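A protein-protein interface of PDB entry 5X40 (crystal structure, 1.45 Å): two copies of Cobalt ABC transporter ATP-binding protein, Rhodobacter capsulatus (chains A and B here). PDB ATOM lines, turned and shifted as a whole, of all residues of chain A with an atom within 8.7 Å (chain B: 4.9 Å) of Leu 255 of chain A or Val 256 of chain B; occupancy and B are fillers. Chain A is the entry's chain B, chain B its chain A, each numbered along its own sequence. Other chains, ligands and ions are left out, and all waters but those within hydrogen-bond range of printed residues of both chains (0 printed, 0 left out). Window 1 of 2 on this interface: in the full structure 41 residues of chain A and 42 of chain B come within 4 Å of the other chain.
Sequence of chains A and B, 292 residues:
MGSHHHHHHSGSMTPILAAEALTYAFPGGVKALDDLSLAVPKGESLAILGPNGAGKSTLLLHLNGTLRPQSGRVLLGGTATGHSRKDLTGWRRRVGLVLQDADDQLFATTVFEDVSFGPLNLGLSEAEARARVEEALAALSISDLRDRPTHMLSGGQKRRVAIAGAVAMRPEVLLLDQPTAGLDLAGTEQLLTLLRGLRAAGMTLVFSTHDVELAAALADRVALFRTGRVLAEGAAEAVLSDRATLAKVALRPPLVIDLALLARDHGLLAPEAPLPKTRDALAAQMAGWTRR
The side-chain carboxylate of Asp 258 of chain A is in salt-bridge range of the guanidinium group of Arg 279 of chain B (2.7 Å).
OD2 of Asp 258 of chain B is in salt-bridge range of NE of Arg 279 of chain A, 2.8 Å away.
Among the printed residues, merely in contact across the chains: Arg 252 of chain A with Arg 279 of chain B (3.2 Å), Leu 255 of chain A with Leu 255 of chain B (3.7 Å), Leu 255 of chain A with Val 256 of chain B (3.6 Å), Leu 255 of chain A with Leu 259 of chain B (3.8 Å), Leu 255 of chain A with Arg 279 of chain B (3.7 Å) and Leu 259 of chain A with Leu 259 of chain B (3.6 Å).
Along chain B the printed residues that touch a printed residue of chain A span positions 255 to 279.
Of the 24 printed residues of chain A, 5 touch a printed residue of chain B.
Hydrophobic or aromatic side chains of chain A within 4 Å of the printed part of chain B: Leu 255 and Leu 259.
Among the printed residues, Asp or Glu carboxylates within 4 Å of a Lys or Arg side-chain nitrogen of the other chain: Asp 258 of chain A with Arg 279 of chain B (2.7 Å) and Arg 279 of chain A with Asp 258 of chain B (2.8 Å).
The guanidinium group of Arg 243 of chain A lies within salt-bridge range of the side-chain carboxylate of Asp 258 of chain A.
N of Val 256 of chain B sits at hydrogen-bond distance from OE2 of Glu 213 of chain B, 2.9 Å away.
The side-chain carboxylate of Glu 213 of chain A sits at hydrogen-bond distance from the backbone NH of Leu 255 of chain A (2.9 Å).
The side-chain carboxylate (OE2) of Glu 213 of chain B lies within hydrogen-bond range of the backbone NH (N) of Leu 255 of chain B (3.0 Å).
Of chain B, only Leu 255 (3.7 Å), Val 256 (3.6 Å), Leu 259 (3.8 Å) and Arg 279 (3.7 Å) come within 4 Å of Leu 255 of chain A.
Of chain A, only Leu 255 (3.6 Å) comes within 4 Å of Val 256 of chain B.
Of the printed residues of chain B, Arg 279 of chain A touches Asp 258.
Of the printed residues of chain A, Leu 259 of chain B touches Leu 255 and Leu 259.
Pro 276 of chain B touches none of the printed residues of chain A.
The nearest residue of chain A that does not touch Val 256 of chain B is Leu 259 of chain A (6.9 Å).
The nearest printed residue of chain A that does not touch Leu 259 of chain B is Arg 279 of chain A (4.004 Å).
Leu 255 of chain A touches Val 256 of chain B, but with the chains exchanged Val 256 of chain A does not touch Leu 255 of chain B (4.4 Å).
Leu 255 of chain A touches Arg 279 of chain B, but with the chains exchanged Arg 279 of chain A does not touch Leu 255 of chain B (4.8 Å).
Asp 258 of chain A touches Arg 279 of chain B, and with the chains exchanged Arg 279 of chain A touches Asp 258 of chain B.
Leu 259 of chain B touches its own counterpart, Leu 259 of chain A.
Positions printed for both chains: 213, 254, 255, 256, 257, 258, 259, 260, 276, 277, 278, 279 and 282.
Of the 8 pairs that touch across the chains among the printed residues, 4 have their exchanged pair printed and touching as well.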
ATOM      1  N   ASP A 211      26.553   3.120  -9.007  1.00  0.00           N
ATOM      2  CA  ASP A 211      25.541   2.196  -8.510  1.00  0.00           C
ATOM      3  C   ASP A 211      26.004   1.618  -7.168  1.00  0.00           C
ATOM      4  O   ASP A 211      26.819   0.695  -7.135  1.00  0.00           O
ATOM      5  CB  ASP A 211      25.293   1.087  -9.542  1.00  0.00           C
ATOM      6  CG  ASP A 211      24.116   0.184  -9.177  1.00  0.00           C
ATOM      7  OD1 ASP A 211      23.707   0.183  -8.000  1.00  0.00           O
ATOM      8  OD2 ASP A 211      23.592  -0.530 -10.069  1.00  0.00           O
ATOM      9  N   VAL A 212      25.497   2.163  -6.060  1.00  0.00           N
ATOM     10  CA  VAL A 212      25.941   1.690  -4.747  1.00  0.00           C
ATOM     11  C   VAL A 212      25.449   0.273  -4.493  1.00  0.00           C
ATOM     12  O   VAL A 212      26.055  -0.459  -3.711  1.00  0.00           O
ATOM     13  CB  VAL A 212      25.495   2.626  -3.588  1.00  0.00           C
ATOM     14  CG1 VAL A 212      26.156   3.997  -3.730  1.00  0.00           C
ATOM     15  CG2 VAL A 212      23.986   2.750  -3.508  1.00  0.00           C
ATOM     16  N   GLU A 213      24.359  -0.126  -5.149  1.00  0.00           N
ATOM     17  CA  GLU A 213      23.882  -1.502  -5.016  1.00  0.00           C
ATOM     18  C   GLU A 213      24.870  -2.464  -5.666  1.00  0.00           C
ATOM     19  O   GLU A 213      25.091  -3.564  -5.166  1.00  0.00           O
ATOM     20  CB  GLU A 213      22.495  -1.691  -5.643  1.00  0.00           C
ATOM     21  CG  GLU A 213      21.462  -0.637  -5.243  1.00  0.00           C
ATOM     22  CD  GLU A 213      21.089  -0.655  -3.769  1.00  0.00           C
ATOM     23  OE1 GLU A 213      21.244  -1.706  -3.102  1.00  0.00           O
ATOM     24  OE2 GLU A 213      20.627   0.396  -3.280  1.00  0.00           O
ATOM     25  N   ALA A 216      27.769  -2.806  -3.317  1.00  0.00           N
ATOM     26  CA  ALA A 216      27.379  -3.692  -2.221  1.00  0.00           C
ATOM     27  C   ALA A 216      27.401  -5.163  -2.641  1.00  0.00           C
ATOM     28  O   ALA A 216      27.784  -6.036  -1.860  1.00  0.00           O
ATOM     29  CB  ALA A 216      26.005  -3.316  -1.708  1.00  0.00           C
ATOM     30  N   LEU A 240      29.991   1.279   3.255  1.00  0.00           N
ATOM     31  CA  LEU A 240      28.647   1.384   2.698  1.00  0.00           C
ATOM     32  C   LEU A 240      27.546   1.520   3.752  1.00  0.00           C
ATOM     33  O   LEU A 240      26.415   1.876   3.415  1.00  0.00           O
ATOM     34  CB  LEU A 240      28.367   0.180   1.792  1.00  0.00           C
ATOM     35  CG  LEU A 240      29.237   0.191   0.519  1.00  0.00           C
ATOM     36  CD1 LEU A 240      28.996  -1.061  -0.328  1.00  0.00           C
ATOM     37  CD2 LEU A 240      29.012   1.461  -0.308  1.00  0.00           C
ATOM     38  N   ARG A 243      26.688   6.362   7.024  1.00  0.00           N
ATOM     39  CA  ARG A 243      25.916   7.426   6.396  1.00  0.00           C
ATOM     40  C   ARG A 243      26.687   8.749   6.315  1.00  0.00           C
ATOM     41  O   ARG A 243      26.691   9.399   5.274  1.00  0.00           O
ATOM     42  CB  ARG A 243      24.599   7.646   7.142  1.00  0.00           C
ATOM     43  CG  ARG A 243      23.678   8.623   6.428  1.00  0.00           C
ATOM     44  CD  ARG A 243      22.412   8.928   7.227  1.00  0.00           C
ATOM     45  NE  ARG A 243      21.615   7.739   7.537  1.00  0.00           N
ATOM     46  CZ  ARG A 243      20.872   7.076   6.657  1.00  0.00           C
ATOM     47  NH1 ARG A 243      20.175   6.013   7.053  1.00  0.00           N
ATOM     48  NH2 ARG A 243      20.838   7.456   5.384  1.00  0.00           N
ATOM     49  N   ARG A 252      24.192   8.056  -0.676  1.00  0.00           N
ATOM     50  CA  ARG A 252      23.456   7.393   0.383  1.00  0.00           C
ATOM     51  C   ARG A 252      23.880   5.931   0.454  1.00  0.00           C
ATOM     52  O   ARG A 252      24.452   5.398  -0.501  1.00  0.00           O
ATOM     53  CB  ARG A 252      21.948   7.508   0.141  1.00  0.00           C
ATOM     54  CG  ARG A 252      21.433   8.937   0.162  1.00  0.00           C
ATOM     55  CD  ARG A 252      19.918   8.969   0.066  1.00  0.00           C
ATOM     56  NE  ARG A 252      19.426   8.370  -1.174  1.00  0.00           N
ATOM     57  CZ  ARG A 252      18.815   9.051  -2.139  1.00  0.00           C
ATOM     58  NH1 ARG A 252      18.619  10.358  -2.010  1.00  0.00           N
ATOM     59  NH2 ARG A 252      18.398   8.425  -3.234  1.00  0.00           N
ATOM     60  N   PRO A 253      23.609   5.271   1.588  1.00  0.00           N
ATOM     61  CA  PRO A 253      23.876   3.829   1.635  1.00  0.00           C
ATOM     62  C   PRO A 253      23.001   3.063   0.641  1.00  0.00           C
ATOM     63  O   PRO A 253      22.006   3.621   0.177  1.00  0.00           O
ATOM     64  CB  PRO A 253      23.514   3.452   3.078  1.00  0.00           C
ATOM     65  CG  PRO A 253      23.596   4.751   3.847  1.00  0.00           C
ATOM     66  CD  PRO A 253      23.133   5.792   2.885  1.00  0.00           C
ATOM     67  N   PRO A 254      23.360   1.806   0.325  1.00  0.00           N
ATOM     68  CA  PRO A 254      22.445   0.937  -0.425  1.00  0.00           C
ATOM     69  C   PRO A 254      21.081   0.946   0.256  1.00  0.00           C
ATOM     70  O   PRO A 254      21.036   1.031   1.481  1.00  0.00           O
ATOM     71  CB  PRO A 254      23.106  -0.438  -0.336  1.00  0.00           C
ATOM     72  CG  PRO A 254      24.549  -0.168  -0.090  1.00  0.00           C
ATOM     73  CD  PRO A 254      24.596   1.105   0.716  1.00  0.00           C
ATOM     74  N   LEU A 255      19.999   0.852  -0.508  1.00  0.00           N
ATOM     75  CA  LEU A 255      18.670   1.148   0.021  1.00  0.00           C
ATOM     76  C   LEU A 255      18.277   0.329   1.257  1.00  0.00           C
ATOM     77  O   LEU A 255      17.801   0.893   2.240  1.00  0.00           O
ATOM     78  CB  LEU A 255      17.622   0.966  -1.073  1.00  0.00           C
ATOM     79  CG  LEU A 255      16.205   1.364  -0.658  1.00  0.00           C
ATOM     80  CD1 LEU A 255      16.139   2.845  -0.309  1.00  0.00           C
ATOM     81  CD2 LEU A 255      15.199   1.011  -1.747  1.00  0.00           C
ATOM     82  N   VAL A 256      18.469  -0.988   1.230  1.00  0.00           N
ATOM     83  CA  VAL A 256      18.091  -1.780   2.400  1.00  0.00           C
ATOM     84  C   VAL A 256      18.905  -1.370   3.629  1.00  0.00           C
ATOM     85  O   VAL A 256      18.347  -1.237   4.708  1.00  0.00           O
ATOM     86  CB  VAL A 256      18.244  -3.297   2.155  1.00  0.00           C
ATOM     87  CG1 VAL A 256      17.972  -4.093   3.445  1.00  0.00           C
ATOM     88  CG2 VAL A 256      17.289  -3.740   1.063  1.00  0.00           C
ATOM     89  N   ILE A 257      20.204  -1.138   3.466  1.00  0.00           N
ATOM     90  CA  ILE A 257      21.039  -0.703   4.585  1.00  0.00           C
ATOM     91  C   ILE A 257      20.606   0.674   5.071  1.00  0.00           C
ATOM     92  O   ILE A 257      20.594   0.945   6.273  1.00  0.00           O
ATOM     93  CB  ILE A 257      22.529  -0.693   4.194  1.00  0.00           C
ATOM     94  CG1 ILE A 257      23.016  -2.136   4.023  1.00  0.00           C
ATOM     95  CG2 ILE A 257      23.373   0.043   5.239  1.00  0.00           C
ATOM     96  CD1 ILE A 257      24.399  -2.246   3.453  1.00  0.00           C
ATOM     97  N   ASP A 258      20.258   1.538   4.127  1.00  0.00           N
ATOM     98  CA  ASP A 258      19.746   2.868   4.427  1.00  0.00           C
ATOM     99  C   ASP A 258      18.570   2.771   5.403  1.00  0.00           C
ATOM    100  O   ASP A 258      18.594   3.339   6.499  1.00  0.00           O
ATOM    101  CB  ASP A 258      19.337   3.546   3.110  1.00  0.00           C
ATOM    102  CG  ASP A 258      19.022   5.019   3.254  1.00  0.00           C
ATOM    103  OD1 ASP A 258      18.931   5.541   4.389  1.00  0.00           O
ATOM    104  OD2 ASP A 258      18.843   5.656   2.195  1.00  0.00           O
ATOM    105  N   LEU A 259      17.560   2.008   5.011  1.00  0.00           N
ATOM    106  CA  LEU A 259      16.328   1.896   5.777  1.00  0.00           C
ATOM    107  C   LEU A 259      16.587   1.202   7.082  1.00  0.00           C
ATOM    108  O   LEU A 259      15.968   1.483   8.109  1.00  0.00           O
ATOM    109  CB  LEU A 259      15.277   1.111   5.003  1.00  0.00           C
ATOM    110  CG  LEU A 259      14.894   1.770   3.695  1.00  0.00           C
ATOM    111  CD1 LEU A 259      13.824   0.970   3.002  1.00  0.00           C
ATOM    112  CD2 LEU A 259      14.426   3.187   3.999  1.00  0.00           C
ATOM    113  N   ALA A 260      17.495   0.249   7.020  1.00  0.00           N
ATOM    114  CA  ALA A 260      17.735  -0.549   8.179  1.00  0.00           C
ATOM    115  C   ALA A 260      18.537   0.236   9.224  1.00  0.00           C
ATOM    116  O   ALA A 260      18.316   0.038  10.426  1.00  0.00           O
ATOM    117  CB  ALA A 260      18.417  -1.836   7.783  1.00  0.00           C
ATOM    118  N   LEU A 261      19.423   1.135   8.793  1.00  0.00           N
ATOM    119  CA  LEU A 261      20.034   2.101   9.706  1.00  0.00           C
ATOM    120  C   LEU A 261      18.974   2.993  10.344  1.00  0.00           C
ATOM    121  O   LEU A 261      19.037   3.291  11.543  1.00  0.00           O
ATOM    122  CB  LEU A 261      21.054   2.961   8.970  1.00  0.00           C
ATOM    123  CG  LEU A 261      22.394   2.302   8.654  1.00  0.00           C
ATOM    124  CD1 LEU A 261      23.176   3.129   7.649  1.00  0.00           C
ATOM    125  CD2 LEU A 261      23.188   2.110   9.932  1.00  0.00           C
ATOM    126  N   LEU A 262      18.016   3.443   9.538  1.00  0.00           N
ATOM    127  CA  LEU A 262      16.893   4.229  10.050  1.00  0.00           C
ATOM    128  C   LEU A 262      16.099   3.454  11.104  1.00  0.00           C
ATOM    129  O   LEU A 262      15.725   3.995  12.152  1.00  0.00           O
ATOM    130  CB  LEU A 262      15.973   4.648   8.900  1.00  0.00           C
ATOM    131  CG  LEU A 262      16.406   5.905   8.146  1.00  0.00           C
ATOM    132  CD1 LEU A 262      15.494   6.173   6.961  1.00  0.00           C
ATOM    133  CD2 LEU A 262      16.408   7.088   9.101  1.00  0.00           C
ATOM    134  N   LEU A 275      22.070  -5.712  11.684  1.00  0.00           N
ATOM    135  CA  LEU A 275      21.453  -4.909  10.658  1.00  0.00           C
ATOM    136  C   LEU A 275      21.063  -5.715   9.430  1.00  0.00           C
ATOM    137  O   LEU A 275      21.907  -6.260   8.754  1.00  0.00           O
ATOM    138  CB  LEU A 275      22.492  -3.935  10.194  1.00  0.00           C
ATOM    139  CG  LEU A 275      22.300  -2.443  10.051  1.00  0.00           C
ATOM    140  CD1 LEU A 275      22.223  -1.957   8.636  1.00  0.00           C
ATOM    141  CD2 LEU A 275      21.338  -1.752  10.981  1.00  0.00           C
ATOM    142  N   PRO A 276      19.785  -5.725   9.129  1.00  0.00           N
ATOM    143  CA  PRO A 276      19.329  -6.331   7.863  1.00  0.00           C
ATOM    144  C   PRO A 276      19.956  -5.650   6.642  1.00  0.00           C
ATOM    145  O   PRO A 276      19.890  -4.426   6.493  1.00  0.00           O
ATOM    146  CB  PRO A 276      17.799  -6.133   7.888  1.00  0.00           C
ATOM    147  CG  PRO A 276      17.533  -5.119   8.940  1.00  0.00           C
ATOM    148  CD  PRO A 276      18.662  -5.215   9.936  1.00  0.00           C
ATOM    149  N   LYS A 277      20.582  -6.443   5.778  1.00  0.00           N
ATOM    150  CA  LYS A 277      21.259  -5.899   4.607  1.00  0.00           C
ATOM    151  C   LYS A 277      20.625  -6.380   3.321  1.00  0.00           C
ATOM    152  O   LYS A 277      20.960  -5.902   2.238  1.00  0.00           O
ATOM    153  CB  LYS A 277      22.735  -6.285   4.619  1.00  0.00           C
ATOM    154  CG  LYS A 277      23.459  -5.860   5.870  1.00  0.00           C
ATOM    155  CD  LYS A 277      24.890  -6.361   5.864  1.00  0.00           C
ATOM    156  CE  LYS A 277      25.492  -6.245   7.245  1.00  0.00           C
ATOM    157  NZ  LYS A 277      25.325  -4.863   7.773  1.00  0.00           N
ATOM    158  N   THR A 278      19.720  -7.347   3.434  1.00  0.00           N
ATOM    159  CA  THR A 278      19.043  -7.874   2.264  1.00  0.00           C
ATOM    160  C   THR A 278      17.544  -7.650   2.347  1.00  0.00           C
ATOM    161  O   THR A 278      16.989  -7.419   3.429  1.00  0.00           O
ATOM    162  CB  THR A 278      19.296  -9.379   2.085  1.00  0.00           C
ATOM    163  OG1 THR A 278      18.784 -10.085   3.223  1.00  0.00           O
ATOM    164  CG2 THR A 278      20.781  -9.662   1.938  1.00  0.00           C
ATOM    165  N   ARG A 279      16.905  -7.713   1.189  1.00  0.00           N
ATOM    166  CA  ARG A 279      15.459  -7.709   1.096  1.00  0.00           C
ATOM    167  C   ARG A 279      14.843  -8.782   1.998  1.00  0.00           C
ATOM    168  O   ARG A 279      13.880  -8.522   2.727  1.00  0.00           O
ATOM    169  CB  ARG A 279      15.046  -7.933  -0.355  1.00  0.00           C
ATOM    170  CG  ARG A 279      13.618  -7.608  -0.644  1.00  0.00           C
ATOM    171  CD  ARG A 279      12.723  -8.837  -0.624  1.00  0.00           C
ATOM    172  NE  ARG A 279      11.424  -8.450  -1.143  1.00  0.00           N
ATOM    173  CZ  ARG A 279      10.268  -9.020  -0.824  1.00  0.00           C
ATOM    174  NH1 ARG A 279       9.154  -8.568  -1.377  1.00  0.00           N
ATOM    175  NH2 ARG A 279      10.219 -10.031   0.039  1.00  0.00           N
ATOM    176  N   LEU A 282      15.166  -7.782   5.683  1.00  0.00           N
ATOM    177  CA  LEU A 282      14.286  -6.681   6.037  1.00  0.00           C
ATOM    178  C   LEU A 282      12.845  -7.171   6.093  1.00  0.00           C
ATOM    179  O   LEU A 282      12.092  -6.792   6.988  1.00  0.00           O
ATOM    180  CB  LEU A 282      14.445  -5.528   5.043  1.00  0.00           C
ATOM    181  CG  LEU A 282      13.681  -4.243   5.348  1.00  0.00           C
ATOM    182  CD1 LEU A 282      14.141  -3.630   6.673  1.00  0.00           C
ATOM    183  CD2 LEU A 282      13.881  -3.264   4.222  1.00  0.00           C
ATOM    184  N   MET A 286       9.990  -6.937   9.220  1.00  0.00           N
ATOM    185  CA  MET A 286       8.715  -6.245   9.069  1.00  0.00           C
ATOM    186  C   MET A 286       7.555  -6.931   9.771  1.00  0.00           C
ATOM    187  O   MET A 286       6.619  -6.270  10.215  1.00  0.00           O
ATOM    188  CB  MET A 286       8.384  -6.093   7.592  1.00  0.00           C
ATOM    189  CG  MET A 286       9.292  -5.129   6.878  1.00  0.00           C
ATOM    190  SD  MET A 286       8.585  -4.645   5.302  1.00  0.00           S
ATOM    191  CE  MET A 286       9.655  -3.293   4.846  1.00  0.00           C
ATOM    192  N   GLU B 213      14.305   2.951 -10.924  1.00  0.00           N
ATOM    193  CA  GLU B 213      14.058   3.907  -9.845  1.00  0.00           C
ATOM    194  C   GLU B 213      13.767   5.296 -10.403  1.00  0.00           C
ATOM    195  O   GLU B 213      12.959   6.046  -9.860  1.00  0.00           O
ATOM    196  CB  GLU B 213      15.254   3.964  -8.897  1.00  0.00           C
ATOM    197  CG  GLU B 213      15.487   2.687  -8.120  1.00  0.00           C
ATOM    198  CD  GLU B 213      14.443   2.473  -7.039  1.00  0.00           C
ATOM    199  OE1 GLU B 213      13.642   3.402  -6.792  1.00  0.00           O
ATOM    200  OE2 GLU B 213      14.420   1.382  -6.438  1.00  0.00           O
ATOM    201  N   PRO B 254      11.138  -1.767  -9.254  1.00  0.00           N
ATOM    202  CA  PRO B 254      12.266  -1.083  -8.610  1.00  0.00           C
ATOM    203  C   PRO B 254      12.310  -1.432  -7.132  1.00  0.00           C
ATOM    204  O   PRO B 254      11.268  -1.730  -6.544  1.00  0.00           O
ATOM    205  CB  PRO B 254      11.981   0.407  -8.839  1.00  0.00           C
ATOM    206  CG  PRO B 254      10.563   0.502  -9.299  1.00  0.00           C
ATOM    207  CD  PRO B 254      10.113  -0.850  -9.779  1.00  0.00           C
ATOM    208  N   LEU B 255      13.506  -1.430  -6.554  1.00  0.00           N
ATOM    209  CA  LEU B 255      13.681  -1.851  -5.172  1.00  0.00           C
ATOM    210  C   LEU B 255      12.766  -1.074  -4.228  1.00  0.00           C
ATOM    211  O   LEU B 255      12.162  -1.664  -3.334  1.00  0.00           O
ATOM    212  CB  LEU B 255      15.145  -1.704  -4.738  1.00  0.00           C
ATOM    213  CG  LEU B 255      15.424  -2.299  -3.352  1.00  0.00           C
ATOM    214  CD1 LEU B 255      14.870  -3.721  -3.255  1.00  0.00           C
ATOM    215  CD2 LEU B 255      16.913  -2.275  -3.030  1.00  0.00           C
ATOM    216  N   VAL B 256      12.653   0.236  -4.429  1.00  0.00           N
ATOM    217  CA  VAL B 256      11.773   1.041  -3.585  1.00  0.00           C
ATOM    218  C   VAL B 256      10.341   0.518  -3.630  1.00  0.00           C
ATOM    219  O   VAL B 256       9.684   0.407  -2.598  1.00  0.00           O
ATOM    220  CB  VAL B 256      11.773   2.528  -3.994  1.00  0.00           C
ATOM    221  CG1 VAL B 256      10.728   3.296  -3.196  1.00  0.00           C
ATOM    222  CG2 VAL B 256      13.138   3.140  -3.761  1.00  0.00           C
ATOM    223  N   ILE B 257       9.868   0.168  -4.825  1.00  0.00           N
ATOM    224  CA  ILE B 257       8.498  -0.313  -4.971  1.00  0.00           C
ATOM    225  C   ILE B 257       8.350  -1.726  -4.419  1.00  0.00           C
ATOM    226  O   ILE B 257       7.335  -2.048  -3.810  1.00  0.00           O
ATOM    227  CB  ILE B 257       8.043  -0.236  -6.446  1.00  0.00           C
ATOM    228  CG1 ILE B 257       7.910   1.239  -6.833  1.00  0.00           C
ATOM    229  CG2 ILE B 257       6.721  -0.961  -6.664  1.00  0.00           C
ATOM    230  CD1 ILE B 257       7.289   1.481  -8.167  1.00  0.00           C
ATOM    231  N   ASP B 258       9.371  -2.559  -4.590  1.00  0.00           N
ATOM    232  CA  ASP B 258       9.339  -3.891  -3.991  1.00  0.00           C
ATOM    233  C   ASP B 258       9.203  -3.770  -2.481  1.00  0.00           C
ATOM    234  O   ASP B 258       8.386  -4.462  -1.872  1.00  0.00           O
ATOM    235  CB  ASP B 258      10.593  -4.697  -4.341  1.00  0.00           C
ATOM    236  CG  ASP B 258      10.608  -6.078  -3.681  1.00  0.00           C
ATOM    237  OD1 ASP B 258       9.568  -6.769  -3.701  1.00  0.00           O
ATOM    238  OD2 ASP B 258      11.661  -6.466  -3.133  1.00  0.00           O
ATOM    239  N   LEU B 259       9.994  -2.881  -1.882  1.00  0.00           N
ATOM    240  CA  LEU B 259       9.969  -2.706  -0.433  1.00  0.00           C
ATOM    241  C   LEU B 259       8.650  -2.082   0.018  1.00  0.00           C
ATOM    242  O   LEU B 259       8.144  -2.407   1.087  1.00  0.00           O
ATOM    243  CB  LEU B 259      11.153  -1.855   0.034  1.00  0.00           C
ATOM    244  CG  LEU B 259      12.548  -2.460  -0.155  1.00  0.00           C
ATOM    245  CD1 LEU B 259      13.610  -1.583   0.494  1.00  0.00           C
ATOM    246  CD2 LEU B 259      12.624  -3.873   0.400  1.00  0.00           C
ATOM    247  N   ALA B 260       8.088  -1.202  -0.807  1.00  0.00           N
ATOM    248  CA  ALA B 260       6.793  -0.598  -0.495  1.00  0.00           C
ATOM    249  C   ALA B 260       5.682  -1.645  -0.552  1.00  0.00           C
ATOM    250  O   ALA B 260       4.788  -1.664   0.293  1.00  0.00           O
ATOM    251  CB  ALA B 260       6.496   0.546  -1.446  1.00  0.00           C
ATOM    252  N   PRO B 276       4.703   4.439  -1.805  1.00  0.00           N
ATOM    253  CA  PRO B 276       5.938   5.227  -1.845  1.00  0.00           C
ATOM    254  C   PRO B 276       6.753   4.853  -3.079  1.00  0.00           C
ATOM    255  O   PRO B 276       6.958   3.665  -3.338  1.00  0.00           O
ATOM    256  CB  PRO B 276       6.657   4.817  -0.558  1.00  0.00           C
ATOM    257  CG  PRO B 276       5.554   4.426   0.370  1.00  0.00           C
ATOM    258  CD  PRO B 276       4.508   3.778  -0.501  1.00  0.00           C
ATOM    259  N   LYS B 277       7.199   5.839  -3.845  1.00  0.00           N
ATOM    260  CA  LYS B 277       7.914   5.517  -5.072  1.00  0.00           C
ATOM    261  C   LYS B 277       9.322   6.115  -5.094  1.00  0.00           C
ATOM    262  O   LYS B 277      10.019   6.048  -6.110  1.00  0.00           O
ATOM    263  CB  LYS B 277       7.106   5.970  -6.296  1.00  0.00           C
ATOM    264  CG  LYS B 277       6.720   7.434  -6.318  1.00  0.00           C
ATOM    265  CD  LYS B 277       5.842   7.766  -7.522  1.00  0.00           C
ATOM    266  CE  LYS B 277       4.565   6.934  -7.557  1.00  0.00           C
ATOM    267  NZ  LYS B 277       3.769   7.219  -8.791  1.00  0.00           N
ATOM    268  N   THR B 278       9.744   6.675  -3.965  1.00  0.00           N
ATOM    269  CA  THR B 278      11.112   7.162  -3.811  1.00  0.00           C
ATOM    270  C   THR B 278      11.665   6.753  -2.454  1.00  0.00           C
ATOM    271  O   THR B 278      10.907   6.424  -1.538  1.00  0.00           O
ATOM    272  CB  THR B 278      11.212   8.693  -3.926  1.00  0.00           C
ATOM    273  OG1 THR B 278      10.505   9.294  -2.836  1.00  0.00           O
ATOM    274  CG2 THR B 278      10.635   9.190  -5.246  1.00  0.00           C
ATOM    275  N   ARG B 279      12.987   6.786  -2.325  1.00  0.00           N
ATOM    276  CA  ARG B 279      13.630   6.502  -1.045  1.00  0.00           C
ATOM    277  C   ARG B 279      13.112   7.388   0.088  1.00  0.00           C
ATOM    278  O   ARG B 279      12.803   6.898   1.169  1.00  0.00           O
ATOM    279  CB  ARG B 279      15.140   6.670  -1.162  1.00  0.00           C
ATOM    280  CG  ARG B 279      15.858   6.497   0.155  1.00  0.00           C
ATOM    281  CD  ARG B 279      16.705   7.711   0.433  1.00  0.00           C
ATOM    282  NE  ARG B 279      17.184   7.743   1.809  1.00  0.00           N
ATOM    283  CZ  ARG B 279      16.649   8.467   2.786  1.00  0.00           C
ATOM    284  NH1 ARG B 279      15.617   9.271   2.550  1.00  0.00           N
ATOM    285  NH2 ARG B 279      17.174   8.408   4.001  1.00  0.00           N
ATOM    286  N   LEU B 282       9.541   6.404   1.146  1.00  0.00           N
ATOM    287  CA  LEU B 282       9.530   5.169   1.911  1.00  0.00           C
ATOM    288  C   LEU B 282      10.060   5.418   3.323  1.00  0.00           C
ATOM    289  O   LEU B 282       9.485   4.950   4.307  1.00  0.00           O
ATOM    290  CB  LEU B 282      10.357   4.104   1.203  1.00  0.00           C
ATOM    291  CG  LEU B 282      10.103   2.658   1.610  1.00  0.00           C
ATOM    292  CD1 LEU B 282       8.614   2.387   1.773  1.00  0.00           C
ATOM    293  CD2 LEU B 282      10.706   1.752   0.557  1.00  0.00           C
